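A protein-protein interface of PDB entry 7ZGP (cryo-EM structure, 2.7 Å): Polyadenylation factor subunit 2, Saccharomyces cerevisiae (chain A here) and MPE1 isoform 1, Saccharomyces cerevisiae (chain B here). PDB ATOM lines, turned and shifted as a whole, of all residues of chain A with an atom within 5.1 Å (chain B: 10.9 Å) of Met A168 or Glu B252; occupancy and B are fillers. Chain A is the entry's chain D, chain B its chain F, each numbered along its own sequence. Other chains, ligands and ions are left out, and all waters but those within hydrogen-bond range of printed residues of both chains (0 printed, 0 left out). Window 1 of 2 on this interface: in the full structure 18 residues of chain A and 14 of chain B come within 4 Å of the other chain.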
ATOM      1  N   LYS A 160     -17.654  28.670  -8.027  1.00  0.00           N
ATOM      2  CA  LYS A 160     -18.435  27.668  -7.321  1.00  0.00           C
ATOM      3  C   LYS A 160     -17.637  26.378  -7.221  1.00  0.00           C
ATOM      4  O   LYS A 160     -17.002  25.953  -8.191  1.00  0.00           O
ATOM      5  CB  LYS A 160     -19.766  27.413  -8.029  1.00  0.00           C
ATOM      6  CG  LYS A 160     -20.740  28.576  -7.947  1.00  0.00           C
ATOM      7  CD  LYS A 160     -22.157  28.139  -8.268  1.00  0.00           C
ATOM      8  CE  LYS A 160     -23.127  29.299  -8.162  1.00  0.00           C
ATOM      9  NZ  LYS A 160     -22.642  30.483  -8.917  1.00  0.00           N
ATOM     10  N   ILE A 161     -17.662  25.764  -6.043  1.00  0.00           N
ATOM     11  CA  ILE A 161     -16.978  24.502  -5.795  1.00  0.00           C
ATOM     12  C   ILE A 161     -18.028  23.402  -5.768  1.00  0.00           C
ATOM     13  O   ILE A 161     -19.000  23.477  -5.009  1.00  0.00           O
ATOM     14  CB  ILE A 161     -16.180  24.544  -4.483  1.00  0.00           C
ATOM     15  CG1 ILE A 161     -14.997  25.503  -4.618  1.00  0.00           C
ATOM     16  CG2 ILE A 161     -15.706  23.153  -4.106  1.00  0.00           C
ATOM     17  CD1 ILE A 161     -14.418  25.952  -3.297  1.00  0.00           C
ATOM     18  N   TRP A 162     -17.835  22.381  -6.598  1.00  0.00           N
ATOM     19  CA  TRP A 162     -18.818  21.328  -6.788  1.00  0.00           C
ATOM     20  C   TRP A 162     -18.254  19.987  -6.343  1.00  0.00           C
ATOM     21  O   TRP A 162     -17.095  19.665  -6.621  1.00  0.00           O
ATOM     22  CB  TRP A 162     -19.250  21.232  -8.254  1.00  0.00           C
ATOM     23  CG  TRP A 162     -19.685  22.530  -8.842  1.00  0.00           C
ATOM     24  CD1 TRP A 162     -18.885  23.507  -9.350  1.00  0.00           C
ATOM     25  CD2 TRP A 162     -21.030  22.994  -8.988  1.00  0.00           C
ATOM     26  NE1 TRP A 162     -19.647  24.555  -9.801  1.00  0.00           N
ATOM     27  CE2 TRP A 162     -20.969  24.264  -9.591  1.00  0.00           C
ATOM     28  CE3 TRP A 162     -22.280  22.459  -8.666  1.00  0.00           C
ATOM     29  CZ2 TRP A 162     -22.108  25.006  -9.879  1.00  0.00           C
ATOM     30  CZ3 TRP A 162     -23.410  23.198  -8.953  1.00  0.00           C
ATOM     31  CH2 TRP A 162     -23.316  24.459  -9.552  1.00  0.00           C
ATOM     32  N   GLN A 163     -19.083  19.216  -5.648  1.00  0.00           N
ATOM     33  CA  GLN A 163     -18.783  17.822  -5.400  1.00  0.00           C
ATOM     34  C   GLN A 163     -19.011  17.019  -6.681  1.00  0.00           C
ATOM     35  O   GLN A 163     -19.692  17.484  -7.597  1.00  0.00           O
ATOM     36  CB  GLN A 163     -19.656  17.294  -4.264  1.00  0.00           C
ATOM     37  CG  GLN A 163     -19.009  17.379  -2.896  1.00  0.00           C
ATOM     38  CD  GLN A 163     -19.934  16.925  -1.786  1.00  0.00           C
ATOM     39  OE1 GLN A 163     -21.150  16.863  -1.963  1.00  0.00           O
ATOM     40  NE2 GLN A 163     -19.361  16.602  -0.634  1.00  0.00           N
ATOM     41  N   PHE A 166     -22.243  16.892  -8.239  1.00  0.00           N
ATOM     42  CA  PHE A 166     -22.742  18.217  -8.607  1.00  0.00           C
ATOM     43  C   PHE A 166     -23.590  18.826  -7.493  1.00  0.00           C
ATOM     44  O   PHE A 166     -24.668  19.376  -7.724  1.00  0.00           O
ATOM     45  CB  PHE A 166     -23.509  18.171  -9.929  1.00  0.00           C
ATOM     46  CG  PHE A 166     -22.635  17.915 -11.117  1.00  0.00           C
ATOM     47  CD1 PHE A 166     -21.936  18.948 -11.712  1.00  0.00           C
ATOM     48  CD2 PHE A 166     -22.496  16.638 -11.627  1.00  0.00           C
ATOM     49  CE1 PHE A 166     -21.126  18.714 -12.800  1.00  0.00           C
ATOM     50  CE2 PHE A 166     -21.685  16.398 -12.714  1.00  0.00           C
ATOM     51  CZ  PHE A 166     -20.998  17.438 -13.300  1.00  0.00           C
ATOM     52  N   SER A 167     -23.043  18.809  -6.276  1.00  0.00           N
ATOM     53  CA  SER A 167     -23.726  19.487  -5.147  1.00  0.00           C
ATOM     54  C   SER A 167     -22.891  20.711  -4.767  1.00  0.00           C
ATOM     55  O   SER A 167     -21.865  20.524  -4.095  1.00  0.00           O
ATOM     56  CB  SER A 167     -23.880  18.562  -3.979  1.00  0.00           C
ATOM     57  OG  SER A 167     -24.452  17.329  -4.385  1.00  0.00           O
ATOM     58  N   MET A 168     -23.290  21.907  -5.211  1.00  0.00           N
ATOM     59  CA  MET A 168     -22.484  23.127  -4.937  1.00  0.00           C
ATOM     60  C   MET A 168     -22.258  23.219  -3.426  1.00  0.00           C
ATOM     61  O   MET A 168     -23.257  23.203  -2.689  1.00  0.00           O
ATOM     62  CB  MET A 168     -23.198  24.383  -5.443  1.00  0.00           C
ATOM     63  CG  MET A 168     -22.267  25.557  -5.665  1.00  0.00           C
ATOM     64  SD  MET A 168     -22.284  26.705  -4.271  1.00  0.00           S
ATOM     65  CE  MET A 168     -24.016  27.165  -4.257  1.00  0.00           C
ATOM     66  N   VAL A 169     -21.000  23.325  -2.987  1.00  0.00           N
ATOM     67  CA  VAL A 169     -20.702  23.285  -1.523  1.00  0.00           C
ATOM     68  C   VAL A 169     -20.106  24.613  -1.058  1.00  0.00           C
ATOM     69  O   VAL A 169     -20.105  24.849   0.164  1.00  0.00           O
ATOM     70  CB  VAL A 169     -19.743  22.122  -1.205  1.00  0.00           C
ATOM     71  CG1 VAL A 169     -20.369  20.769  -1.502  1.00  0.00           C
ATOM     72  CG2 VAL A 169     -18.422  22.271  -1.940  1.00  0.00           C
ATOM     73  N   LYS A 170     -19.624  25.446  -1.980  1.00  0.00           N
ATOM     74  CA  LYS A 170     -18.944  26.670  -1.578  1.00  0.00           C
ATOM     75  C   LYS A 170     -18.958  27.666  -2.727  1.00  0.00           C
ATOM     76  O   LYS A 170     -18.621  27.313  -3.861  1.00  0.00           O
ATOM     77  CB  LYS A 170     -17.504  26.377  -1.144  1.00  0.00           C
ATOM     78  CG  LYS A 170     -16.688  27.612  -0.816  1.00  0.00           C
ATOM     79  CD  LYS A 170     -16.693  27.892   0.676  1.00  0.00           C
ATOM     80  CE  LYS A 170     -15.676  28.958   1.040  1.00  0.00           C
ATOM     81  NZ  LYS A 170     -15.886  29.473   2.420  1.00  0.00           N
ATOM     82  N   GLU A 171     -19.345  28.901  -2.426  1.00  0.00           N
ATOM     83  CA  GLU A 171     -19.331  30.000  -3.380  1.00  0.00           C
ATOM     84  C   GLU A 171     -18.305  31.040  -2.959  1.00  0.00           C
ATOM     85  O   GLU A 171     -18.174  31.352  -1.771  1.00  0.00           O
ATOM     86  CB  GLU A 171     -20.702  30.675  -3.485  1.00  0.00           C
ATOM     87  CG  GLU A 171     -21.694  29.987  -4.388  1.00  0.00           C
ATOM     88  CD  GLU A 171     -23.075  30.602  -4.294  1.00  0.00           C
ATOM     89  OE1 GLU A 171     -23.314  31.383  -3.350  1.00  0.00           O
ATOM     90  OE2 GLU A 171     -23.922  30.307  -5.163  1.00  0.00           O
ATOM     91  N   GLY B 213     -31.915  22.296 -12.258  1.00  0.00           N
ATOM     92  CA  GLY B 213     -31.422  21.146 -11.534  1.00  0.00           C
ATOM     93  C   GLY B 213     -31.345  21.297 -10.036  1.00  0.00           C
ATOM     94  O   GLY B 213     -30.886  20.377  -9.354  1.00  0.00           O
ATOM     95  N   ILE B 214     -31.778  22.427  -9.499  1.00  0.00           N
ATOM     96  CA  ILE B 214     -31.588  22.714  -8.077  1.00  0.00           C
ATOM     97  C   ILE B 214     -32.733  22.078  -7.293  1.00  0.00           C
ATOM     98  O   ILE B 214     -33.904  22.375  -7.575  1.00  0.00           O
ATOM     99  CB  ILE B 214     -31.533  24.216  -7.850  1.00  0.00           C
ATOM    100  CG1 ILE B 214     -30.505  24.834  -8.799  1.00  0.00           C
ATOM    101  CG2 ILE B 214     -31.114  24.498  -6.424  1.00  0.00           C
ATOM    102  CD1 ILE B 214     -30.340  26.323  -8.649  1.00  0.00           C
ATOM    103  N   PRO B 215     -32.450  21.211  -6.317  1.00  0.00           N
ATOM    104  CA  PRO B 215     -33.529  20.428  -5.697  1.00  0.00           C
ATOM    105  C   PRO B 215     -34.285  21.143  -4.587  1.00  0.00           C
ATOM    106  O   PRO B 215     -34.548  20.547  -3.539  1.00  0.00           O
ATOM    107  CB  PRO B 215     -32.794  19.198  -5.143  1.00  0.00           C
ATOM    108  CG  PRO B 215     -31.367  19.306  -5.617  1.00  0.00           C
ATOM    109  CD  PRO B 215     -31.121  20.742  -5.904  1.00  0.00           C
ATOM    110  N   LYS B 217     -34.307  22.602  -2.076  1.00  0.00           N
ATOM    111  CA  LYS B 217     -33.889  22.735  -0.690  1.00  0.00           C
ATOM    112  C   LYS B 217     -32.662  23.613  -0.526  1.00  0.00           C
ATOM    113  O   LYS B 217     -32.372  24.043   0.594  1.00  0.00           O
ATOM    114  CB  LYS B 217     -33.612  21.357  -0.070  1.00  0.00           C
ATOM    115  CG  LYS B 217     -32.178  20.879  -0.209  1.00  0.00           C
ATOM    116  CD  LYS B 217     -31.960  19.582   0.551  1.00  0.00           C
ATOM    117  CE  LYS B 217     -31.443  19.852   1.954  1.00  0.00           C
ATOM    118  NZ  LYS B 217     -30.683  18.697   2.503  1.00  0.00           N
ATOM    119  N   PHE B 218     -32.014  23.935  -1.654  1.00  0.00           N
ATOM    120  CA  PHE B 218     -30.855  24.865  -1.650  1.00  0.00           C
ATOM    121  C   PHE B 218     -31.344  26.209  -2.194  1.00  0.00           C
ATOM    122  O   PHE B 218     -30.498  27.055  -2.537  1.00  0.00           O
ATOM    123  CB  PHE B 218     -29.709  24.274  -2.472  1.00  0.00           C
ATOM    124  CG  PHE B 218     -29.379  22.842  -2.138  1.00  0.00           C
ATOM    125  CD1 PHE B 218     -28.599  22.530  -1.036  1.00  0.00           C
ATOM    126  CD2 PHE B 218     -29.855  21.803  -2.921  1.00  0.00           C
ATOM    127  CE1 PHE B 218     -28.301  21.212  -0.728  1.00  0.00           C
ATOM    128  CE2 PHE B 218     -29.554  20.486  -2.612  1.00  0.00           C
ATOM    129  CZ  PHE B 218     -28.779  20.193  -1.517  1.00  0.00           C
ATOM    130  N   LEU B 219     -32.664  26.388  -2.294  1.00  0.00           N
ATOM    131  CA  LEU B 219     -33.274  27.632  -2.741  1.00  0.00           C
ATOM    132  C   LEU B 219     -34.055  28.249  -1.592  1.00  0.00           C
ATOM    133  O   LEU B 219     -34.917  27.592  -0.998  1.00  0.00           O
ATOM    134  CB  LEU B 219     -34.209  27.397  -3.929  1.00  0.00           C
ATOM    135  CG  LEU B 219     -33.651  26.717  -5.176  1.00  0.00           C
ATOM    136  CD1 LEU B 219     -34.785  26.217  -6.049  1.00  0.00           C
ATOM    137  CD2 LEU B 219     -32.769  27.684  -5.947  1.00  0.00           C
ATOM    138  N   LYS B 220     -33.755  29.506  -1.282  1.00  0.00           N
ATOM    139  CA  LYS B 220     -34.504  30.273  -0.298  1.00  0.00           C
ATOM    140  C   LYS B 220     -35.183  31.444  -0.990  1.00  0.00           C
ATOM    141  O   LYS B 220     -34.620  32.042  -1.914  1.00  0.00           O
ATOM    142  CB  LYS B 220     -33.603  30.784   0.829  1.00  0.00           C
ATOM    143  CG  LYS B 220     -32.403  31.582   0.357  1.00  0.00           C
ATOM    144  CD  LYS B 220     -31.530  32.005   1.525  1.00  0.00           C
ATOM    145  CE  LYS B 220     -31.978  33.341   2.089  1.00  0.00           C
ATOM    146  NZ  LYS B 220     -31.169  34.464   1.542  1.00  0.00           N
ATOM    147  N   ILE B 241     -33.356  34.757 -10.543  1.00  0.00           N
ATOM    148  CA  ILE B 241     -33.672  33.356 -10.808  1.00  0.00           C
ATOM    149  C   ILE B 241     -34.969  33.020 -10.085  1.00  0.00           C
ATOM    150  O   ILE B 241     -35.144  33.352  -8.910  1.00  0.00           O
ATOM    151  CB  ILE B 241     -32.509  32.424 -10.389  1.00  0.00           C
ATOM    152  CG1 ILE B 241     -32.940  30.959 -10.412  1.00  0.00           C
ATOM    153  CG2 ILE B 241     -31.990  32.790  -9.016  1.00  0.00           C
ATOM    154  CD1 ILE B 241     -31.851  30.010  -9.957  1.00  0.00           C
ATOM    155  N   VAL B 249     -33.134  32.005  -4.608  1.00  0.00           N
ATOM    156  CA  VAL B 249     -31.701  32.100  -4.860  1.00  0.00           C
ATOM    157  C   VAL B 249     -31.049  30.815  -4.373  1.00  0.00           C
ATOM    158  O   VAL B 249     -31.485  30.209  -3.391  1.00  0.00           O
ATOM    159  CB  VAL B 249     -31.082  33.347  -4.183  1.00  0.00           C
ATOM    160  CG1 VAL B 249     -31.122  33.216  -2.670  1.00  0.00           C
ATOM    161  CG2 VAL B 249     -29.653  33.556  -4.658  1.00  0.00           C
ATOM    162  N   GLN B 250     -30.005  30.386  -5.077  1.00  0.00           N
ATOM    163  CA  GLN B 250     -29.279  29.187  -4.684  1.00  0.00           C
ATOM    164  C   GLN B 250     -28.336  29.490  -3.530  1.00  0.00           C
ATOM    165  O   GLN B 250     -27.658  30.523  -3.521  1.00  0.00           O
ATOM    166  CB  GLN B 250     -28.494  28.609  -5.860  1.00  0.00           C
ATOM    167  CG  GLN B 250     -28.438  27.090  -5.854  1.00  0.00           C
ATOM    168  CD  GLN B 250     -27.147  26.546  -6.428  1.00  0.00           C
ATOM    169  OE1 GLN B 250     -26.396  27.265  -7.087  1.00  0.00           O
ATOM    170  NE2 GLN B 250     -26.880  25.269  -6.181  1.00  0.00           N
ATOM    171  N   VAL B 251     -28.300  28.571  -2.561  1.00  0.00           N
ATOM    172  CA  VAL B 251     -27.392  28.728  -1.389  1.00  0.00           C
ATOM    173  C   VAL B 251     -26.438  27.531  -1.369  1.00  0.00           C
ATOM    174  O   VAL B 251     -26.877  26.424  -1.739  1.00  0.00           O
ATOM    175  CB  VAL B 251     -28.194  28.826  -0.077  1.00  0.00           C
ATOM    176  CG1 VAL B 251     -29.160  29.999  -0.102  1.00  0.00           C
ATOM    177  CG2 VAL B 251     -28.935  27.534   0.232  1.00  0.00           C
ATOM    178  N   GLU B 252     -25.185  27.745  -0.963  1.00  0.00           N
ATOM    179  CA  GLU B 252     -24.211  26.628  -0.861  1.00  0.00           C
ATOM    180  C   GLU B 252     -24.729  25.625   0.170  1.00  0.00           C
ATOM    181  O   GLU B 252     -25.333  26.073   1.163  1.00  0.00           O
ATOM    182  CB  GLU B 252     -22.849  27.159  -0.423  1.00  0.00           C
ATOM    183  CG  GLU B 252     -22.550  28.555  -0.933  1.00  0.00           C
ATOM    184  CD  GLU B 252     -21.337  29.202  -0.286  1.00  0.00           C
ATOM    185  OE1 GLU B 252     -20.566  28.479   0.373  1.00  0.00           O
ATOM    186  OE2 GLU B 252     -21.173  30.428  -0.434  1.00  0.00           O
ATOM    187  N   ASP B 253     -24.522  24.324  -0.059  1.00  0.00           N
ATOM    188  CA  ASP B 253     -24.899  23.338   0.988  1.00  0.00           C
ATOM    189  C   ASP B 253     -23.808  23.395   2.061  1.00  0.00           C
ATOM    190  O   ASP B 253     -22.900  22.544   2.032  1.00  0.00           O
ATOM    191  CB  ASP B 253     -25.172  21.940   0.417  1.00  0.00           C
ATOM    192  CG  ASP B 253     -23.971  21.251  -0.205  1.00  0.00           C
ATOM    193  OD1 ASP B 253     -22.967  21.935  -0.446  1.00  0.00           O
ATOM    194  OD2 ASP B 253     -24.055  20.029  -0.437  1.00  0.00           O
ATOM    195  N   LYS B 254     -23.889  24.378   2.964  1.00  0.00           N
ATOM    196  CA  LYS B 254     -22.830  24.560   3.993  1.00  0.00           C
ATOM    197  C   LYS B 254     -22.886  23.395   4.983  1.00  0.00           C
ATOM    198  O   LYS B 254     -22.828  23.655   6.198  1.00  0.00           O
ATOM    199  CB  LYS B 254     -23.009  25.909   4.696  1.00  0.00           C
ATOM    200  N   GLN B 255     -23.017  22.168   4.481  1.00  0.00           N
ATOM    201  CA  GLN B 255     -22.996  20.968   5.353  1.00  0.00           C
ATOM    202  C   GLN B 255     -21.988  19.996   4.742  1.00  0.00           C
ATOM    203  O   GLN B 255     -21.147  19.470   5.489  1.00  0.00           O
ATOM    204  CB  GLN B 255     -24.388  20.344   5.448  1.00  0.00           C
ATOM    205  CG  GLN B 255     -24.417  19.053   6.253  1.00  0.00           C
ATOM    206  CD  GLN B 255     -25.801  18.456   6.323  1.00  0.00           C
ATOM    207  OE1 GLN B 255     -26.754  18.981   5.751  1.00  0.00           O
ATOM    208  NE2 GLN B 255     -25.922  17.344   7.030  1.00  0.00           N
ATOM    209  N   SER B 256     -22.067  19.795   3.426  1.00  0.00           N
ATOM    210  CA  SER B 256     -21.084  18.925   2.731  1.00  0.00           C
ATOM    211  C   SER B 256     -19.692  19.547   2.861  1.00  0.00           C
ATOM    212  O   SER B 256     -18.733  18.797   3.116  1.00  0.00           O
ATOM    213  CB  SER B 256     -21.465  18.729   1.290  1.00  0.00           C
ATOM    214  OG  SER B 256     -22.757  18.150   1.186  1.00  0.00           O
ATOM    215  N   TRP B 257     -19.599  20.869   2.707  1.00  0.00           N
ATOM    216  CA  TRP B 257     -18.294  21.564   2.856  1.00  0.00           C
ATOM    217  C   TRP B 257     -17.801  21.397   4.295  1.00  0.00           C
ATOM    218  O   TRP B 257     -16.595  21.153   4.479  1.00  0.00           O
ATOM    219  CB  TRP B 257     -18.413  23.042   2.467  1.00  0.00           C
ATOM    220  CG  TRP B 257     -17.094  23.744   2.387  1.00  0.00           C
ATOM    221  CD1 TRP B 257     -16.618  24.705   3.230  1.00  0.00           C
ATOM    222  CD2 TRP B 257     -16.065  23.529   1.405  1.00  0.00           C
ATOM    223  NE1 TRP B 257     -15.370  25.107   2.838  1.00  0.00           N
ATOM    224  CE2 TRP B 257     -15.004  24.403   1.721  1.00  0.00           C
ATOM    225  CE3 TRP B 257     -15.939  22.689   0.293  1.00  0.00           C
ATOM    226  CZ2 TRP B 257     -13.835  24.456   0.963  1.00  0.00           C
ATOM    227  CZ3 TRP B 257     -14.784  22.743  -0.455  1.00  0.00           C
ATOM    228  CH2 TRP B 257     -13.749  23.616  -0.122  1.00  0.00           C
ATOM    229  N   GLU B 258     -18.707  21.518   5.268  1.00  0.00           N
ATOM    230  CA  GLU B 258     -18.331  21.365   6.698  1.00  0.00           C
ATOM    231  C   GLU B 258     -17.846  19.934   6.941  1.00  0.00           C
ATOM    232  O   GLU B 258     -16.802  19.773   7.595  1.00  0.00           O
ATOM    233  CB  GLU B 258     -19.519  21.711   7.594  1.00  0.00           C
ATOM    234  CG  GLU B 258     -19.954  23.159   7.475  1.00  0.00           C
ATOM    235  CD  GLU B 258     -21.044  23.572   8.448  1.00  0.00           C
ATOM    236  OE1 GLU B 258     -21.535  22.696   9.186  1.00  0.00           O
ATOM    237  OE2 GLU B 258     -21.398  24.767   8.464  1.00  0.00           O
ATOM    238  N   TYR B 260     -16.503  17.994   4.815  1.00  0.00           N
ATOM    239  CA  TYR B 260     -15.164  17.967   4.180  1.00  0.00           C
ATOM    240  C   TYR B 260     -14.160  18.565   5.165  1.00  0.00           C
ATOM    241  O   TYR B 260     -13.046  18.023   5.296  1.00  0.00           O
ATOM    242  CB  TYR B 260     -15.183  18.738   2.860  1.00  0.00           C
ATOM    243  CG  TYR B 260     -13.827  19.162   2.356  1.00  0.00           C
ATOM    244  CD1 TYR B 260     -12.878  18.226   1.982  1.00  0.00           C
ATOM    245  CD2 TYR B 260     -13.496  20.502   2.243  1.00  0.00           C
ATOM    246  CE1 TYR B 260     -11.633  18.608   1.514  1.00  0.00           C
ATOM    247  CE2 TYR B 260     -12.255  20.902   1.776  1.00  0.00           C
ATOM    248  CZ  TYR B 260     -11.320  19.951   1.410  1.00  0.00           C
ATOM    249  OH  TYR B 260     -10.095  20.336   0.949  1.00  0.00           O
ATOM    250  N   GLN B 261     -14.556  19.648   5.838  1.00  0.00           N
ATOM    251  CA  GLN B 261     -13.672  20.283   6.845  1.00  0.00           C
ATOM    252  C   GLN B 261     -13.466  19.294   7.996  1.00  0.00           C
ATOM    253  O   GLN B 261     -12.302  19.079   8.388  1.00  0.00           O
ATOM    254  CB  GLN B 261     -14.280  21.598   7.333  1.00  0.00           C
ATOM    255  CG  GLN B 261     -14.571  22.582   6.213  1.00  0.00           C
ATOM    256  CD  GLN B 261     -13.343  22.890   5.393  1.00  0.00           C
ATOM    257  OE1 GLN B 261     -12.222  22.906   5.895  1.00  0.00           O
ATOM    258  NE2 GLN B 261     -13.550  23.148   4.112  1.00  0.00           N
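O of Met A168 is in hydrogen-bond range of N of Asp B253, 3.1 Å away.
The backbone NH (N) of Glu A171 sits close to the side-chain carboxylate (OE1) of Glu B252.
The backbone carbonyl oxygen of Lys A160 sits close to the indole nitrogen of Trp A162, at 3.4 Å.
The side-chain amino group of Lys A160 lies within salt-bridge range of the side-chain carboxylate of Glu A171, at 3.97 Å.
O of Ile A161 sits at hydrogen-bond distance from N of Val A169, at 2.8 Å.
The backbone NH (N) of Val B251 lies within hydrogen-bond range of the backbone carbonyl oxygen (O) of Phe B218.
The side-chain carboxylate (OD2) of Asp B253 sits at hydrogen-bond distance from the side-chain hydroxyl (OG) of Ser B256, at 2.8 Å.
NE1 of Trp B257 sits close to NE2 of Gln B261 (3.0 Å).
Among the printed residues, merely in contact across the chains: Val A169 with Asp B253, Lys A170 with Glu B252, Val A169 with Trp B257, Met A168 with Glu B252, Gln A163 with Ser B256, Val A169 with Ser B256, Val A169 with Glu B252, Met A168 with Gln B250, Lys A170 with Trp B257, Met A168 with Val B251, Ile A161 with Trp B257, Ser A167 with Asp B253 and Lys A160 with Gln B250.
Of chain B, only Gln B250 (3.7 Å), Val B251 (3.8 Å), Glu B252 (3.4 Å) and Asp B253 (2.6 Å) come within 4 Å of Met A168.
Glu B252 touches just these residues of chain A: Met A168 (3.4 Å), Val A169 (3.6 Å), Lys A170 (3.1 Å) and Glu A171 (2.9 Å).
No residue of chain B comes within 4 Å of Trp A162.
Val A169 touches four residues of chain B.
Lys A170 touches two residues of chain B.
Of chain B, only Glu B252 comes within 4 Å of Glu A171.
Of the printed residues of chain A, Gln B250 touches Lys A160 and Met A168.
Printed residues of chain B within 4 Å of Lys A160: Gln B250 (3.997 Å).
Of the printed residues of chain B, Ile A161 touches Trp B257.
Of the printed residues of chain A, Ser B256 touches Gln A163 (3.6 Å) and Val A169 (3.6 Å).
Of the printed residues of chain A, Val B251 touches Met A168.
Ile B241 touches none of the printed residues of chain A.
Ile B214 touches none of the printed residues of chain A.
The nearest printed residue of chain B that does not touch Lys A160 is Glu B252 (7.2 Å).
Printed residues of chain A that touch a printed residue of chain B: Lys A160, Ile A161, Gln A163, Ser A167, Met A168, Val A169, Lys A170 and Glu A171.
Hydrophobic or aromatic side chains of chain A within 4 Å of the printed part of chain B: Ile A161, Met A168 and Val A169.
Printed residues of chain B that touch a printed residue of chain A: Gln B250, Val B251, Glu B252, Asp B253, Ser B256 and Trp B257.
Hydrophobic or aromatic side chains of chain B that line the printed part of chain A: Trp B257.
Along chain B the printed residues that touch a printed residue of chain A span positions 250 to 257.
Among the printed residues, 15 pairs touch across the chains.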
